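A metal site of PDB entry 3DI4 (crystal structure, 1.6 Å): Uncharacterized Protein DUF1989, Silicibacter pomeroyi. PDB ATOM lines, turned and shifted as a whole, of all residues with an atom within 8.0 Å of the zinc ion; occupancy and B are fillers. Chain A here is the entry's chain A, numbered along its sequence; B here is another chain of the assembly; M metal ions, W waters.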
ATOM      1  N   GLN A  78     -13.854 -16.147   3.095  1.00  0.00           N
ATOM      2  CA  GLN A  78     -12.878 -17.041   2.549  1.00  0.00           C
ATOM      3  C   GLN A  78     -11.860 -16.294   1.679  1.00  0.00           C
ATOM      4  O   GLN A  78     -12.257 -15.474   0.827  1.00  0.00           O
ATOM      5  CB  GLN A  78     -13.621 -18.108   1.702  1.00  0.00           C
ATOM      6  CG  GLN A  78     -12.745 -19.028   0.853  1.00  0.00           C
ATOM      7  CD  GLN A  78     -11.965 -20.010   1.662  1.00  0.00           C
ATOM      8  OE1 GLN A  78     -12.539 -20.755   2.484  1.00  0.00           O
ATOM      9  NE2 GLN A  78     -10.638 -20.029   1.476  1.00  0.00           N
ATOM     10  N   VAL A  79     -10.598 -16.596   1.881  1.00  0.00           N
ATOM     11  CA  VAL A  79      -9.570 -15.951   1.059  1.00  0.00           C
ATOM     12  C   VAL A  79      -9.207 -16.810  -0.156  1.00  0.00           C
ATOM     13  O   VAL A  79      -9.336 -18.049  -0.157  1.00  0.00           O
ATOM     14  CB  VAL A  79      -8.326 -15.547   1.910  1.00  0.00           C
ATOM     15  CG1 VAL A  79      -8.790 -14.783   3.202  1.00  0.00           C
ATOM     16  CG2 VAL A  79      -7.503 -16.756   2.273  1.00  0.00           C
ATOM     17  N   GLY A  80      -8.696 -16.148  -1.188  1.00  0.00           N
ATOM     18  CA  GLY A  80      -8.356 -16.797  -2.440  1.00  0.00           C
ATOM     19  C   GLY A  80      -6.933 -16.465  -2.829  1.00  0.00           C
ATOM     20  O   GLY A  80      -6.441 -15.358  -2.568  1.00  0.00           O
ATOM     21  N   ASP A  81      -6.263 -17.455  -3.400  1.00  0.00           N
ATOM     22  CA  ASP A  81      -4.897 -17.258  -3.865  1.00  0.00           C
ATOM     23  C   ASP A  81      -4.917 -17.330  -5.366  1.00  0.00           C
ATOM     24  O   ASP A  81      -5.269 -18.371  -5.955  1.00  0.00           O
ATOM     25  CB  ASP A  81      -4.010 -18.366  -3.340  1.00  0.00           C
ATOM     26  CG  ASP A  81      -3.618 -18.194  -1.931  1.00  0.00           C
ATOM     27  OD1 ASP A  81      -4.422 -17.676  -1.131  1.00  0.00           O
ATOM     28  OD2 ASP A  81      -2.488 -18.616  -1.616  1.00  0.00           O
ATOM     29  N   THR A 149       3.554 -15.774  -0.176  1.00  0.00           N
ATOM     30  CA  THR A 149       3.891 -16.577  -1.369  1.00  0.00           C
ATOM     31  C   THR A 149       2.744 -17.483  -1.806  1.00  0.00           C
ATOM     32  O   THR A 149       2.412 -17.563  -2.977  1.00  0.00           O
ATOM     33  CB  THR A 149       5.158 -17.396  -1.108  1.00  0.00           C
ATOM     34  OG1 THR A 149       4.977 -18.195   0.047  1.00  0.00           O
ATOM     35  CG2 THR A 149       6.299 -16.429  -0.863  1.00  0.00           C
ATOM     36  N   ARG A 150       2.193 -18.157  -0.817  1.00  0.00           N
ATOM     37  CA  ARG A 150       1.106 -19.106  -0.909  1.00  0.00           C
ATOM     38  C   ARG A 150       1.400 -20.171   0.121  1.00  0.00           C
ATOM     39  O   ARG A 150       2.570 -20.560   0.308  1.00  0.00           O
ATOM     40  CB  ARG A 150       0.959 -19.788  -2.274  1.00  0.00           C
ATOM     41  CG  ARG A 150       2.175 -20.537  -2.735  1.00  0.00           C
ATOM     42  CD  ARG A 150       2.131 -20.752  -4.229  1.00  0.00           C
ATOM     43  NE  ARG A 150       3.358 -21.262  -4.810  1.00  0.00           N
ATOM     44  CZ  ARG A 150       4.427 -20.519  -5.032  1.00  0.00           C
ATOM     45  NH1 ARG A 150       4.463 -19.232  -4.680  1.00  0.00           N
ATOM     46  NH2 ARG A 150       5.460 -21.070  -5.617  1.00  0.00           N
ATOM     47  N   CYS A 151       0.376 -20.655   0.784  1.00  0.00           N
ATOM     48  CA  CYS A 151       0.593 -21.792   1.683  1.00  0.00           C
ATOM     49  C   CYS A 151       0.988 -22.967   0.820  1.00  0.00           C
ATOM     50  O   CYS A 151       0.547 -23.112  -0.329  1.00  0.00           O
ATOM     51  CB  CYS A 151      -0.625 -22.070   2.591  1.00  0.00           C
ATOM     52  SG  CYS A 151      -2.142 -22.735   1.912  1.00  0.00           S
ATOM     53  N   ASP A 152       1.867 -23.807   1.361  1.00  0.00           N
ATOM     54  CA  ASP A 152       2.466 -24.829   0.517  1.00  0.00           C
ATOM     55  C   ASP A 152       2.872 -26.045   1.377  1.00  0.00           C
ATOM     56  O   ASP A 152       3.105 -25.901   2.606  1.00  0.00           O
ATOM     57  CB  ASP A 152       3.665 -24.260  -0.260  1.00  0.00           C
ATOM     58  CG  ASP A 152       4.921 -24.219   0.557  1.00  0.00           C
ATOM     59  OD1 ASP A 152       5.578 -25.285   0.713  1.00  0.00           O
ATOM     60  OD2 ASP A 152       5.209 -23.135   1.054  1.00  0.00           O
ATOM     61  N   HIS A 166      -3.723 -30.140   0.149  1.00  0.00           N
ATOM     62  CA  HIS A 166      -4.664 -29.099  -0.267  1.00  0.00           C
ATOM     63  C   HIS A 166      -4.259 -27.702   0.117  1.00  0.00           C
ATOM     64  O   HIS A 166      -5.115 -26.819   0.252  1.00  0.00           O
ATOM     65  CB  HIS A 166      -6.085 -29.454   0.183  1.00  0.00           C
ATOM     66  CG  HIS A 166      -6.608 -30.625  -0.572  1.00  0.00           C
ATOM     67  ND1 HIS A 166      -7.486 -30.498  -1.619  1.00  0.00           N
ATOM     68  CD2 HIS A 166      -6.287 -31.943  -0.494  1.00  0.00           C
ATOM     69  CE1 HIS A 166      -7.724 -31.696  -2.129  1.00  0.00           C
ATOM     70  NE2 HIS A 166      -7.002 -32.588  -1.471  1.00  0.00           N
ATOM     71  N   CYS A 167      -2.948 -27.510   0.301  1.00  0.00           N
ATOM     72  CA  CYS A 167      -2.420 -26.150   0.387  1.00  0.00           C
ATOM     73  C   CYS A 167      -2.604 -25.476  -0.981  1.00  0.00           C
ATOM     74  O   CYS A 167      -2.691 -26.145  -2.015  1.00  0.00           O
ATOM     75  CB  CYS A 167      -0.913 -26.121   0.714  1.00  0.00           C
ATOM     76  SG  CYS A 167      -0.537 -26.741   2.321  1.00  0.00           S
ATOM     77  N   CYS A 168      -2.588 -24.149  -1.025  1.00  0.00           N
ATOM     78  CA  CYS A 168      -2.823 -23.445  -2.257  1.00  0.00           C
ATOM     79  C   CYS A 168      -1.813 -23.777  -3.341  1.00  0.00           C
ATOM     80  O   CYS A 168      -2.158 -23.866  -4.496  1.00  0.00           O
ATOM     81  CB  CYS A 168      -2.876 -21.940  -2.010  1.00  0.00           C
ATOM     82  SG  CYS A 168      -4.338 -21.419  -1.077  1.00  0.00           S
ATOM     83  N   HIS A 169      -0.549 -23.947  -2.955  1.00  0.00           N
ATOM     84  CA  HIS A 169       0.455 -24.331  -3.950  1.00  0.00           C
ATOM     85  C   HIS A 169       0.031 -25.612  -4.696  1.00  0.00           C
ATOM     86  O   HIS A 169       0.141 -25.684  -5.928  1.00  0.00           O
ATOM     87  CB  HIS A 169       1.820 -24.527  -3.276  1.00  0.00           C
ATOM     88  CG  HIS A 169       2.859 -25.043  -4.210  1.00  0.00           C
ATOM     89  ND1 HIS A 169       3.483 -24.239  -5.136  1.00  0.00           N
ATOM     90  CD2 HIS A 169       3.396 -26.278  -4.367  1.00  0.00           C
ATOM     91  CE1 HIS A 169       4.343 -24.960  -5.832  1.00  0.00           C
ATOM     92  NE2 HIS A 169       4.303 -26.199  -5.390  1.00  0.00           N
ATOM     93  N   ASN A 171      -3.101 -26.945  -4.811  1.00  0.00           N
ATOM     94  CA  ASN A 171      -4.385 -26.732  -5.481  1.00  0.00           C
ATOM     95  C   ASN A 171      -4.179 -26.040  -6.838  1.00  0.00           C
ATOM     96  O   ASN A 171      -4.818 -26.403  -7.854  1.00  0.00           O
ATOM     97  CB  ASN A 171      -5.277 -25.880  -4.625  1.00  0.00           C
ATOM     98  CG  ASN A 171      -5.595 -26.494  -3.271  1.00  0.00           C
ATOM     99  OD1 ASN A 171      -5.446 -27.713  -3.062  1.00  0.00           O
ATOM    100  ND2 ASN A 171      -6.074 -25.657  -2.346  1.00  0.00           N
ATOM    101  N   LEU A 172      -3.302 -25.044  -6.857  1.00  0.00           N
ATOM    102  CA  LEU A 172      -2.953 -24.334  -8.115  1.00  0.00           C
ATOM    103  C   LEU A 172      -2.250 -25.301  -9.069  1.00  0.00           C
ATOM    104  O   LEU A 172      -2.523 -25.313 -10.272  1.00  0.00           O
ATOM    105  CB  LEU A 172      -2.059 -23.132  -7.820  1.00  0.00           C
ATOM    106  CG  LEU A 172      -2.728 -22.006  -7.025  1.00  0.00           C
ATOM    107  CD1 LEU A 172      -1.735 -21.039  -6.422  1.00  0.00           C
ATOM    108  CD2 LEU A 172      -3.747 -21.272  -7.933  1.00  0.00           C
ATOM    109  N   VAL A 194       1.479 -15.528  -5.123  1.00  0.00           N
ATOM    110  CA  VAL A 194       0.057 -15.229  -5.400  1.00  0.00           C
ATOM    111  C   VAL A 194      -0.342 -13.784  -5.082  1.00  0.00           C
ATOM    112  O   VAL A 194       0.330 -13.034  -4.371  1.00  0.00           O
ATOM    113  CB  VAL A 194      -0.836 -16.173  -4.589  1.00  0.00           C
ATOM    114  CG1 VAL A 194      -0.590 -17.634  -4.957  1.00  0.00           C
ATOM    115  CG2 VAL A 194      -0.625 -15.948  -3.043  1.00  0.00           C
ATOM    116  N   ASN A 196      -3.140 -12.504  -2.804  1.00  0.00           N
ATOM    117  CA  ASN A 196      -3.922 -13.057  -1.692  1.00  0.00           C
ATOM    118  C   ASN A 196      -5.229 -12.277  -1.558  1.00  0.00           C
ATOM    119  O   ASN A 196      -5.385 -11.381  -0.739  1.00  0.00           O
ATOM    120  CB  ASN A 196      -3.108 -12.968  -0.426  1.00  0.00           C
ATOM    121  CG  ASN A 196      -2.158 -14.152  -0.256  1.00  0.00           C
ATOM    122  OD1 ASN A 196      -2.598 -15.294  -0.221  1.00  0.00           O
ATOM    123  ND2 ASN A 196      -0.854 -13.888  -0.142  1.00  0.00           N
ATOM    124  N   MET A 199      -7.360 -11.537   1.717  1.00  0.00           N
ATOM    125  CA  MET A 199      -6.586 -11.862   2.915  1.00  0.00           C
ATOM    126  C   MET A 199      -6.161 -10.575   3.562  1.00  0.00           C
ATOM    127  O   MET A 199      -5.730  -9.630   2.884  1.00  0.00           O
ATOM    128  CB  MET A 199      -5.368 -12.782   2.640  1.00  0.00           C
ATOM    129  CG  MET A 199      -4.854 -13.625   3.848  1.00  0.00           C
ATOM    130  SD  MET A 199      -3.279 -14.500   3.232  1.00  0.00           S
ATOM    131  CE  MET A 199      -2.691 -15.103   4.929  1.00  0.00           C
ATOM    132  N   SER A 236      -7.171 -20.532  -6.064  1.00  0.00           N
ATOM    133  CA  SER A 236      -7.332 -21.515  -4.985  1.00  0.00           C
ATOM    134  C   SER A 236      -8.107 -20.963  -3.791  1.00  0.00           C
ATOM    135  O   SER A 236      -7.819 -19.866  -3.313  1.00  0.00           O
ATOM    136  CB  SER A 236      -5.945 -21.970  -4.508  1.00  0.00           C
ATOM    137  OG  SER A 236      -6.082 -22.782  -3.361  1.00  0.00           O
ATOM    138  N   ALA A 237      -9.120 -21.716  -3.327  1.00  0.00           N
ATOM    139  CA  ALA A 237      -9.815 -21.370  -2.106  1.00  0.00           C
ATOM    140  C   ALA A 237      -9.022 -21.962  -0.933  1.00  0.00           C
ATOM    141  O   ALA A 237      -9.034 -23.170  -0.705  1.00  0.00           O
ATOM    142  CB  ALA A 237     -11.241 -21.906  -2.129  1.00  0.00           C
ATOM    143  N   CYS A 238      -8.269 -21.091  -0.276  1.00  0.00           N
ATOM    144  CA  CYS A 238      -7.227 -21.482   0.681  1.00  0.00           C
ATOM    145  C   CYS A 238      -7.775 -22.298   1.860  1.00  0.00           C
ATOM    146  O   CYS A 238      -8.806 -21.939   2.400  1.00  0.00           O
ATOM    147  CB  CYS A 238      -6.619 -20.227   1.278  1.00  0.00           C
ATOM    148  SG  CYS A 238      -5.284 -20.390   2.470  1.00  0.00           S
ATOM    149  N   PRO A 239      -7.042 -23.352   2.303  1.00  0.00           N
ATOM    150  CA  PRO A 239      -7.551 -24.120   3.446  1.00  0.00           C
ATOM    151  C   PRO A 239      -7.534 -23.340   4.750  1.00  0.00           C
ATOM    152  O   PRO A 239      -8.090 -23.833   5.747  1.00  0.00           O
ATOM    153  CB  PRO A 239      -6.604 -25.318   3.539  1.00  0.00           C
ATOM    154  CG  PRO A 239      -5.342 -24.811   2.902  1.00  0.00           C
ATOM    155  CD  PRO A 239      -5.838 -23.966   1.745  1.00  0.00           C
ATOM    156  N   GLY A 240      -6.956 -22.144   4.753  1.00  0.00           N
ATOM    157  CA  GLY A 240      -7.010 -21.248   5.895  1.00  0.00           C
ATOM    158  C   GLY A 240      -8.388 -20.597   6.131  1.00  0.00           C
ATOM    159  O   GLY A 240      -8.623 -19.912   7.138  1.00  0.00           O
ATOM    160  N   GLY A 241      -9.307 -20.781   5.196  1.00  0.00           N
ATOM    161  CA  GLY A 241     -10.627 -20.132   5.268  1.00  0.00           C
ATOM    162  C   GLY A 241     -10.492 -18.608   5.282  1.00  0.00           C
ATOM    163  O   GLY A 241      -9.968 -18.008   4.338  1.00  0.00           O
ATOM    164  N   CYS A 243      -8.692 -17.118   7.395  1.00  0.00           N
ATOM    165  CA  CYS A 243      -7.395 -16.902   8.042  1.00  0.00           C
ATOM    166  C   CYS A 243      -7.547 -16.256   9.469  1.00  0.00           C
ATOM    167  O   CYS A 243      -6.697 -15.476   9.938  1.00  0.00           O
ATOM    168  CB  CYS A 243      -6.445 -16.165   7.057  1.00  0.00           C
ATOM    169  SG  CYS A 243      -5.995 -17.214   5.693  1.00  0.00           S
ATOM    170  N   TYR B  25       4.103 -17.511  10.799  1.00  0.00           N
ATOM    171  CA  TYR B  25       5.097 -18.506  11.112  1.00  0.00           C
ATOM    172  C   TYR B  25       5.859 -18.075  12.357  1.00  0.00           C
ATOM    173  O   TYR B  25       6.883 -17.407  12.295  1.00  0.00           O
ATOM    174  CB  TYR B  25       6.007 -18.684   9.882  1.00  0.00           C
ATOM    175  CG  TYR B  25       5.254 -19.149   8.652  1.00  0.00           C
ATOM    176  CD1 TYR B  25       4.854 -20.492   8.527  1.00  0.00           C
ATOM    177  CD2 TYR B  25       4.931 -18.280   7.606  1.00  0.00           C
ATOM    178  CE1 TYR B  25       4.169 -20.955   7.400  1.00  0.00           C
ATOM    179  CE2 TYR B  25       4.268 -18.740   6.460  1.00  0.00           C
ATOM    180  CZ  TYR B  25       3.890 -20.083   6.369  1.00  0.00           C
ATOM    181  OH  TYR B  25       3.219 -20.550   5.245  1.00  0.00           O
HETATM  182 ZN    ZN M   1      -3.491 -21.004   1.079  1.00  0.00          ZN
HETATM  183  O   HOH W   1      -2.200 -19.422   0.790  1.00  0.00           O
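The backbone NH of Asp 81 sits at hydrogen-bond distance from the backbone carbonyl oxygen of Ser 236, at 2.9 Å. SG of Cys 168 sits close to OD2 of Asp 81, at 3.4 Å. The backbone carbonyl oxygen (O) of Cys 238 is in hydrogen-bond range of the side-chain amide nitrogen (NE2) of Gln 78, at 2.8 Å. The backbone carbonyl oxygen (O) of Cys 151 lies within hydrogen-bond range of the backbone NH (N) of His 169, 3.0 Å away. The side-chain sulfur of Cys 168 lies close to the side-chain hydroxyl of Ser 236. The backbone NH (N) of Cys 238 lies within hydrogen-bond range of the backbone carbonyl oxygen (O) of Val 79 (3.2 Å). The side-chain sulfur (SG) of Cys 238 sits close to the backbone NH (N) of Gly 240 (3.3 Å). The side-chain amide oxygen of Asn 196 lies close to the side-chain carboxylate of Asp 81.
Residues that only touch the zinc ion: Asp 81 (3.7 Å) and Pro 239 (3.8 Å). Within 4 Å of the zinc ion: Asp 81, Cys 151, Cys 168, Cys 238 and Pro 239.
Water W1 is bound to the zinc ion, at 2.1 Å. The zinc ion is bound by SG of Cys 151 (2.3 Å). The zinc ion is bound by SG of Cys 238 (2.4 Å). SG of Cys 168 is bound to the zinc ion (2.4 Å).
Water W1 lies within hydrogen-bond range of OD2 of Asp 81 (2.6 Å) and N of Cys 151 (2.9 Å).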
